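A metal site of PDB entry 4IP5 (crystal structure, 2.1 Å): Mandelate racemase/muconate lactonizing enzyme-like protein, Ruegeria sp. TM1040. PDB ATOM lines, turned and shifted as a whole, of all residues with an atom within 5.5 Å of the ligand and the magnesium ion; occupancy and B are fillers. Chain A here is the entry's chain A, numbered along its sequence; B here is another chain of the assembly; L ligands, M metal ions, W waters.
The side-chain carboxylate (OE1) of Glu 380 is in hydrogen-bond range of the backbone NH (N) of Ala 350 (2.8 Å). The side-chain amide nitrogen of Asn 248 sits at hydrogen-bond distance from the side-chain carboxylate of Asp 24, at 3.4 Å. OD2 of Asp 246 lies close to NZ of Lys 218, at 2.6 Å. The backbone NH (N) of Asn 27 lies within hydrogen-bond range of the side-chain carboxylate (OD1) of Asp 24 (2.5 Å). NZ of Lys 216 lies within salt-bridge range of OE2 of Glu 380. The indole nitrogen (NE1) of Trp 99 of chain B lies within hydrogen-bond range of the backbone carbonyl oxygen (O) of Phe 52 (3.1 Å). NZ of Lys 218 is in hydrogen-bond range of OD1 of Asn 248 (2.8 Å). The side-chain carboxylate (OE2) of Glu 380 sits at hydrogen-bond distance from the side-chain hydroxyl (OG1) of Thr 188 (2.6 Å).
O3 of the ligand is in hydrogen-bond range of NE2 of His 349 (2.8 Å). The side-chain hydroxyl (OH) of Tyr 32 sits at hydrogen-bond distance from an oxygen (O1) of the ligand (2.7 Å). The backbone carbonyl oxygen (O) of Gly 22 sits at hydrogen-bond distance from an oxygen (O1) of the ligand (2.6 Å). NZ of Lys 216 lies close to O5 of the ligand, at 2.7 Å. ND2 of Asn 248 sits close to O4 of the ligand (2.9 Å). NZ of Lys 218 is in hydrogen-bond range of O2 of the ligand. The side-chain carboxylate of Asp 24 sits at hydrogen-bond distance from an oxygen (O2) of the ligand (2.7 Å).
The magnesium ion is bound by O5 of the ligand (2.0 Å). The magnesium ion is bound by water W1 (2.1 Å). The side-chain carboxylate (OD2) of Asp 246 is bound to the magnesium ion, at 2.1 Å. OE2 of Glu 272 binds the magnesium ion, 2.1 Å away. The magnesium ion is bound by OE1 of Glu 299. An oxygen (O4) of the ligand binds the magnesium ion (2.1 Å).
Water W1 lies within hydrogen-bond range of the side-chain carboxylate of Glu 273, the side-chain carboxylate of Asp 246 and the side-chain amide nitrogen of Asn 248. Water W3 lies within hydrogen-bond range of O of Ala 350, OE2 of Glu 380 and N1 of the ligand. Water W2 lies within hydrogen-bond range of the side-chain carboxylate of Glu 380, the side-chain amino group of Lys 216 and the side-chain hydroxyl of Tyr 186.
Trp 192 touches the ligand (CZ3 to O2, 3.4 Å). OE2 of Glu 380 touches O5 of the ligand (3.6 Å). Trp 99 of chain B touches the ligand (CH2 to O3, 3.4 Å). Hydrophobic or aromatic side chains within 4 Å of the ligand: Tyr 32, Trp 192, His 349 and Trp 99 of chain B. The nearest printed residue that does not touch the ligand is Pro 30 (4.3 Å).
Lys 216 touches the magnesium ion (NZ to MG, 3.9 Å). Lys 218 touches the magnesium ion. Five residues have an atom within 4 Å of the magnesium ion: Lys 216, Lys 218, Asp 246, Glu 272 and Glu 299.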
ATOM      1  N   GLY A  22      20.001  13.214 -32.171  1.00  0.00           N
ATOM      2  CA  GLY A  22      20.560  13.986 -31.073  1.00  0.00           C
ATOM      3  C   GLY A  22      22.078  14.032 -31.044  1.00  0.00           C
ATOM      4  O   GLY A  22      22.663  14.814 -30.291  1.00  0.00           O
ATOM      5  N   SER A  23      22.717  13.192 -31.863  1.00  0.00           N
ATOM      6  CA  SER A  23      24.184  13.066 -31.811  1.00  0.00           C
ATOM      7  C   SER A  23      24.920  14.355 -32.194  1.00  0.00           C
ATOM      8  O   SER A  23      24.499  15.059 -33.112  1.00  0.00           O
ATOM      9  CB  SER A  23      24.651  11.922 -32.721  1.00  0.00           C
ATOM     10  OG  SER A  23      24.193  12.115 -34.055  1.00  0.00           O
ATOM     11  N   ASP A  24      26.000  14.648 -31.489  1.00  0.00           N
ATOM     12  CA  ASP A  24      26.795  15.841 -31.782  1.00  0.00           C
ATOM     13  C   ASP A  24      28.279  15.615 -31.472  1.00  0.00           C
ATOM     14  O   ASP A  24      28.686  14.506 -31.130  1.00  0.00           O
ATOM     15  CB  ASP A  24      26.251  17.036 -30.995  1.00  0.00           C
ATOM     16  CG  ASP A  24      26.285  16.801 -29.496  1.00  0.00           C
ATOM     17  OD1 ASP A  24      27.400  16.627 -28.947  1.00  0.00           O
ATOM     18  OD2 ASP A  24      25.202  16.802 -28.864  1.00  0.00           O
ATOM     19  N   ASN A  27      28.435  14.800 -27.626  1.00  0.00           N
ATOM     20  CA  ASN A  27      27.572  13.703 -27.212  1.00  0.00           C
ATOM     21  C   ASN A  27      27.285  12.806 -28.404  1.00  0.00           C
ATOM     22  O   ASN A  27      26.348  13.049 -29.172  1.00  0.00           O
ATOM     23  CB  ASN A  27      26.255  14.273 -26.644  1.00  0.00           C
ATOM     24  CG  ASN A  27      26.492  15.447 -25.688  1.00  0.00           C
ATOM     25  OD1 ASN A  27      27.083  15.260 -24.625  1.00  0.00           O
ATOM     26  ND2 ASN A  27      26.053  16.637 -26.075  1.00  0.00           N
ATOM     27  N   PRO A  30      23.597  10.124 -27.465  1.00  0.00           N
ATOM     28  CA  PRO A  30      22.695  10.433 -26.357  1.00  0.00           C
ATOM     29  C   PRO A  30      21.433   9.569 -26.376  1.00  0.00           C
ATOM     30  O   PRO A  30      20.878   9.290 -27.447  1.00  0.00           O
ATOM     31  CB  PRO A  30      22.334  11.899 -26.604  1.00  0.00           C
ATOM     32  CG  PRO A  30      22.497  12.079 -28.087  1.00  0.00           C
ATOM     33  CD  PRO A  30      23.680  11.226 -28.446  1.00  0.00           C
ATOM     34  N   TYR A  32      17.990  10.183 -25.082  1.00  0.00           N
ATOM     35  CA  TYR A  32      17.087  11.209 -24.581  1.00  0.00           C
ATOM     36  C   TYR A  32      16.265  10.726 -23.396  1.00  0.00           C
ATOM     37  O   TYR A  32      15.532   9.733 -23.497  1.00  0.00           O
ATOM     38  CB  TYR A  32      16.196  11.740 -25.709  1.00  0.00           C
ATOM     39  CG  TYR A  32      16.880  12.752 -26.596  1.00  0.00           C
ATOM     40  CD1 TYR A  32      18.271  12.906 -26.582  1.00  0.00           C
ATOM     41  CD2 TYR A  32      16.143  13.578 -27.447  1.00  0.00           C
ATOM     42  CE1 TYR A  32      18.899  13.851 -27.391  1.00  0.00           C
ATOM     43  CE2 TYR A  32      16.763  14.510 -28.264  1.00  0.00           C
ATOM     44  CZ  TYR A  32      18.133  14.651 -28.224  1.00  0.00           C
ATOM     45  OH  TYR A  32      18.748  15.600 -29.015  1.00  0.00           O
ATOM     46  N   PHE A  52      15.386  17.459 -18.547  1.00  0.00           N
ATOM     47  CA  PHE A  52      15.924  16.642 -19.642  1.00  0.00           C
ATOM     48  C   PHE A  52      17.387  16.257 -19.448  1.00  0.00           C
ATOM     49  O   PHE A  52      18.217  17.124 -19.131  1.00  0.00           O
ATOM     50  CB  PHE A  52      15.747  17.395 -20.969  1.00  0.00           C
ATOM     51  CG  PHE A  52      16.545  16.811 -22.118  1.00  0.00           C
ATOM     52  CD1 PHE A  52      16.174  15.585 -22.678  1.00  0.00           C
ATOM     53  CD2 PHE A  52      17.641  17.487 -22.640  1.00  0.00           C
ATOM     54  CE1 PHE A  52      16.910  15.037 -23.723  1.00  0.00           C
ATOM     55  CE2 PHE A  52      18.373  16.948 -23.695  1.00  0.00           C
ATOM     56  CZ  PHE A  52      18.001  15.719 -24.238  1.00  0.00           C
ATOM     57  N   ILE A  54      20.498  13.037 -21.018  1.00  0.00           N
ATOM     58  CA  ILE A  54      20.777  12.166 -22.166  1.00  0.00           C
ATOM     59  C   ILE A  54      21.187  10.745 -21.779  1.00  0.00           C
ATOM     60  O   ILE A  54      21.968  10.110 -22.485  1.00  0.00           O
ATOM     61  CB  ILE A  54      21.802  12.791 -23.131  1.00  0.00           C
ATOM     62  CG1 ILE A  54      23.104  13.147 -22.392  1.00  0.00           C
ATOM     63  CG2 ILE A  54      21.221  14.047 -23.801  1.00  0.00           C
ATOM     64  CD1 ILE A  54      24.262  13.537 -23.320  1.00  0.00           C
ATOM     65  N   TYR A 186      13.142  27.498 -35.956  1.00  0.00           N
ATOM     66  CA  TYR A 186      14.111  26.856 -36.826  1.00  0.00           C
ATOM     67  C   TYR A 186      14.151  25.374 -36.545  1.00  0.00           C
ATOM     68  O   TYR A 186      13.620  24.925 -35.533  1.00  0.00           O
ATOM     69  CB  TYR A 186      15.509  27.467 -36.680  1.00  0.00           C
ATOM     70  CG  TYR A 186      16.271  27.113 -35.405  1.00  0.00           C
ATOM     71  CD1 TYR A 186      17.045  25.950 -35.333  1.00  0.00           C
ATOM     72  CD2 TYR A 186      16.273  27.972 -34.311  1.00  0.00           C
ATOM     73  CE1 TYR A 186      17.777  25.643 -34.192  1.00  0.00           C
ATOM     74  CE2 TYR A 186      17.012  27.679 -33.161  1.00  0.00           C
ATOM     75  CZ  TYR A 186      17.750  26.525 -33.106  1.00  0.00           C
ATOM     76  OH  TYR A 186      18.464  26.231 -31.957  1.00  0.00           O
ATOM     77  N   THR A 188      16.445  21.678 -36.227  1.00  0.00           N
ATOM     78  CA  THR A 188      17.718  20.989 -36.049  1.00  0.00           C
ATOM     79  C   THR A 188      17.579  19.546 -36.534  1.00  0.00           C
ATOM     80  O   THR A 188      18.511  18.733 -36.462  1.00  0.00           O
ATOM     81  CB  THR A 188      18.132  21.010 -34.558  1.00  0.00           C
ATOM     82  OG1 THR A 188      17.952  22.338 -34.040  1.00  0.00           O
ATOM     83  CG2 THR A 188      19.609  20.591 -34.370  1.00  0.00           C
ATOM     84  N   TRP A 192      21.931  16.447 -37.061  1.00  0.00           N
ATOM     85  CA  TRP A 192      22.679  15.573 -36.149  1.00  0.00           C
ATOM     86  C   TRP A 192      23.937  14.978 -36.778  1.00  0.00           C
ATOM     87  O   TRP A 192      23.929  14.556 -37.939  1.00  0.00           O
ATOM     88  CB  TRP A 192      21.781  14.481 -35.541  1.00  0.00           C
ATOM     89  CG  TRP A 192      20.519  15.058 -34.928  1.00  0.00           C
ATOM     90  CD1 TRP A 192      19.238  14.824 -35.330  1.00  0.00           C
ATOM     91  CD2 TRP A 192      20.429  15.970 -33.822  1.00  0.00           C
ATOM     92  NE1 TRP A 192      18.359  15.536 -34.548  1.00  0.00           N
ATOM     93  CE2 TRP A 192      19.069  16.248 -33.608  1.00  0.00           C
ATOM     94  CE3 TRP A 192      21.380  16.588 -32.995  1.00  0.00           C
ATOM     95  CZ2 TRP A 192      18.625  17.099 -32.596  1.00  0.00           C
ATOM     96  CZ3 TRP A 192      20.936  17.425 -31.985  1.00  0.00           C
ATOM     97  CH2 TRP A 192      19.574  17.670 -31.790  1.00  0.00           C
ATOM     98  N   LYS A 216      19.739  24.232 -38.553  1.00  0.00           N
ATOM     99  CA  LYS A 216      20.955  24.139 -37.741  1.00  0.00           C
ATOM    100  C   LYS A 216      21.666  22.802 -37.930  1.00  0.00           C
ATOM    101  O   LYS A 216      21.028  21.761 -38.030  1.00  0.00           O
ATOM    102  CB  LYS A 216      20.659  24.397 -36.261  1.00  0.00           C
ATOM    103  CG  LYS A 216      21.921  24.545 -35.388  1.00  0.00           C
ATOM    104  CD  LYS A 216      21.597  25.008 -33.969  1.00  0.00           C
ATOM    105  CE  LYS A 216      20.889  23.918 -33.164  1.00  0.00           C
ATOM    106  NZ  LYS A 216      20.583  24.372 -31.769  1.00  0.00           N
ATOM    107  N   LYS A 218      25.141  20.220 -36.788  1.00  0.00           N
ATOM    108  CA  LYS A 218      26.210  19.933 -35.851  1.00  0.00           C
ATOM    109  C   LYS A 218      27.577  19.974 -36.550  1.00  0.00           C
ATOM    110  O   LYS A 218      27.699  19.570 -37.713  1.00  0.00           O
ATOM    111  CB  LYS A 218      25.992  18.574 -35.199  1.00  0.00           C
ATOM    112  CG  LYS A 218      24.751  18.495 -34.325  1.00  0.00           C
ATOM    113  CD  LYS A 218      24.776  19.594 -33.271  1.00  0.00           C
ATOM    114  CE  LYS A 218      23.582  19.492 -32.347  1.00  0.00           C
ATOM    115  NZ  LYS A 218      23.641  20.436 -31.197  1.00  0.00           N
ATOM    116  N   ASP A 246      26.520  24.315 -34.595  1.00  0.00           N
ATOM    117  CA  ASP A 246      26.586  24.056 -33.159  1.00  0.00           C
ATOM    118  C   ASP A 246      27.735  23.103 -32.897  1.00  0.00           C
ATOM    119  O   ASP A 246      27.734  21.992 -33.440  1.00  0.00           O
ATOM    120  CB  ASP A 246      25.273  23.404 -32.714  1.00  0.00           C
ATOM    121  CG  ASP A 246      25.140  23.304 -31.191  1.00  0.00           C
ATOM    122  OD1 ASP A 246      26.138  23.499 -30.445  1.00  0.00           O
ATOM    123  OD2 ASP A 246      24.009  23.015 -30.742  1.00  0.00           O
ATOM    124  N   ASN A 248      28.716  22.253 -29.648  1.00  0.00           N
ATOM    125  CA  ASN A 248      28.493  21.585 -28.365  1.00  0.00           C
ATOM    126  C   ASN A 248      29.682  21.619 -27.400  1.00  0.00           C
ATOM    127  O   ASN A 248      30.004  20.616 -26.763  1.00  0.00           O
ATOM    128  CB  ASN A 248      27.990  20.143 -28.608  1.00  0.00           C
ATOM    129  CG  ASN A 248      26.543  20.112 -29.072  1.00  0.00           C
ATOM    130  OD1 ASN A 248      26.268  20.139 -30.276  1.00  0.00           O
ATOM    131  ND2 ASN A 248      25.620  20.105 -28.122  1.00  0.00           N
ATOM    132  N   GLU A 272      27.060  28.026 -32.283  1.00  0.00           N
ATOM    133  CA  GLU A 272      26.441  27.798 -30.973  1.00  0.00           C
ATOM    134  C   GLU A 272      27.388  27.024 -30.073  1.00  0.00           C
ATOM    135  O   GLU A 272      28.038  26.060 -30.515  1.00  0.00           O
ATOM    136  CB  GLU A 272      25.120  27.035 -31.145  1.00  0.00           C
ATOM    137  CG  GLU A 272      24.538  26.504 -29.834  1.00  0.00           C
ATOM    138  CD  GLU A 272      23.128  25.962 -30.003  1.00  0.00           C
ATOM    139  OE1 GLU A 272      22.457  26.336 -30.998  1.00  0.00           O
ATOM    140  OE2 GLU A 272      22.691  25.169 -29.137  1.00  0.00           O
ATOM    141  N   GLU A 273      27.469  27.435 -28.810  1.00  0.00           N
ATOM    142  CA  GLU A 273      28.386  26.807 -27.847  1.00  0.00           C
ATOM    143  C   GLU A 273      29.774  26.487 -28.433  1.00  0.00           C
ATOM    144  O   GLU A 273      30.179  25.316 -28.509  1.00  0.00           O
ATOM    145  CB  GLU A 273      27.764  25.531 -27.298  1.00  0.00           C
ATOM    146  CG  GLU A 273      26.501  25.757 -26.477  1.00  0.00           C
ATOM    147  CD  GLU A 273      26.345  24.663 -25.433  1.00  0.00           C
ATOM    148  OE1 GLU A 273      25.923  23.544 -25.810  1.00  0.00           O
ATOM    149  OE2 GLU A 273      26.654  24.906 -24.246  1.00  0.00           O
ATOM    150  N   GLU A 299      22.102  26.723 -23.604  1.00  0.00           N
ATOM    151  CA  GLU A 299      21.318  25.529 -23.276  1.00  0.00           C
ATOM    152  C   GLU A 299      21.806  24.851 -21.996  1.00  0.00           C
ATOM    153  O   GLU A 299      21.010  24.243 -21.276  1.00  0.00           O
ATOM    154  CB  GLU A 299      21.285  24.530 -24.435  1.00  0.00           C
ATOM    155  CG  GLU A 299      22.561  23.727 -24.626  1.00  0.00           C
ATOM    156  CD  GLU A 299      22.468  22.817 -25.841  1.00  0.00           C
ATOM    157  OE1 GLU A 299      22.330  23.339 -26.976  1.00  0.00           O
ATOM    158  OE2 GLU A 299      22.510  21.588 -25.669  1.00  0.00           O
ATOM    159  N   HIS A 349      16.622  26.990 -26.641  1.00  0.00           N
ATOM    160  CA  HIS A 349      17.037  25.638 -26.941  1.00  0.00           C
ATOM    161  C   HIS A 349      15.827  24.729 -26.754  1.00  0.00           C
ATOM    162  O   HIS A 349      15.026  24.935 -25.844  1.00  0.00           O
ATOM    163  CB  HIS A 349      18.143  25.224 -25.974  1.00  0.00           C
ATOM    164  CG  HIS A 349      18.456  23.758 -25.995  1.00  0.00           C
ATOM    165  ND1 HIS A 349      18.097  22.912 -24.959  1.00  0.00           N
ATOM    166  CD2 HIS A 349      19.125  22.998 -26.890  1.00  0.00           C
ATOM    167  CE1 HIS A 349      18.525  21.687 -25.239  1.00  0.00           C
ATOM    168  NE2 HIS A 349      19.148  21.715 -26.406  1.00  0.00           N
ATOM    169  N   ALA A 350      15.718  23.721 -27.618  1.00  0.00           N
ATOM    170  CA  ALA A 350      14.583  22.800 -27.547  1.00  0.00           C
ATOM    171  C   ALA A 350      14.984  21.390 -27.953  1.00  0.00           C
ATOM    172  O   ALA A 350      16.152  21.003 -27.820  1.00  0.00           O
ATOM    173  CB  ALA A 350      13.421  23.308 -28.410  1.00  0.00           C
ATOM    174  N   GLU A 380      13.981  27.072 -31.252  1.00  0.00           N
ATOM    175  CA  GLU A 380      14.441  25.819 -31.825  1.00  0.00           C
ATOM    176  C   GLU A 380      13.258  24.859 -31.929  1.00  0.00           C
ATOM    177  O   GLU A 380      12.341  24.889 -31.095  1.00  0.00           O
ATOM    178  CB  GLU A 380      15.552  25.191 -30.982  1.00  0.00           C
ATOM    179  CG  GLU A 380      16.104  23.902 -31.581  1.00  0.00           C
ATOM    180  CD  GLU A 380      17.352  23.377 -30.883  1.00  0.00           C
ATOM    181  OE1 GLU A 380      17.638  23.791 -29.721  1.00  0.00           O
ATOM    182  OE2 GLU A 380      18.065  22.550 -31.501  1.00  0.00           O
ATOM    183  N   TRP B  99      26.369  15.886 -18.786  1.00  0.00           N
ATOM    184  CA  TRP B  99      25.111  16.614 -18.944  1.00  0.00           C
ATOM    185  C   TRP B  99      24.562  17.072 -17.595  1.00  0.00           C
ATOM    186  O   TRP B  99      23.892  18.109 -17.494  1.00  0.00           O
ATOM    187  CB  TRP B  99      24.076  15.737 -19.637  1.00  0.00           C
ATOM    188  CG  TRP B  99      22.937  16.542 -20.134  1.00  0.00           C
ATOM    189  CD1 TRP B  99      21.836  16.932 -19.432  1.00  0.00           C
ATOM    190  CD2 TRP B  99      22.815  17.100 -21.450  1.00  0.00           C
ATOM    191  NE1 TRP B  99      21.012  17.699 -20.245  1.00  0.00           N
ATOM    192  CE2 TRP B  99      21.588  17.812 -21.486  1.00  0.00           C
ATOM    193  CE3 TRP B  99      23.598  17.036 -22.609  1.00  0.00           C
ATOM    194  CZ2 TRP B  99      21.146  18.472 -22.631  1.00  0.00           C
ATOM    195  CZ3 TRP B  99      23.152  17.702 -23.748  1.00  0.00           C
ATOM    196  CH2 TRP B  99      21.944  18.400 -23.744  1.00  0.00           C
HETATM  197  O1  LIG L   1      21.333  16.155 -28.475  1.00  0.00           O
HETATM  198  C1  LIG L   1      22.003  16.977 -27.580  1.00  0.00           C
HETATM  199  C2  LIG L   1      22.448  18.322 -28.101  1.00  0.00           C
HETATM  200  O2  LIG L   1      22.964  18.166 -29.374  1.00  0.00           O
HETATM  201  C3  LIG L   1      21.325  19.355 -28.104  1.00  0.00           C
HETATM  202  O3  LIG L   1      20.928  19.561 -26.781  1.00  0.00           O
HETATM  203  C4  LIG L   1      21.768  20.674 -28.677  1.00  0.00           C
HETATM  204  O4  LIG L   1      22.926  21.056 -28.570  1.00  0.00           O
HETATM  205  N1  LIG L   1      20.817  21.517 -29.346  1.00  0.00           N
HETATM  206  O5  LIG L   1      21.212  22.665 -29.819  1.00  0.00           O
HETATM  207 MG    MG M   1      22.977  23.116 -28.957  1.00  0.00          MG
HETATM  208  O   HOH W   1      24.851  23.236 -28.125  1.00  0.00           O
HETATM  209  O   HOH W   2      19.738  25.541 -28.899  1.00  0.00           O
HETATM  210  O   HOH W   3      18.151  20.465 -29.533  1.00  0.00           O
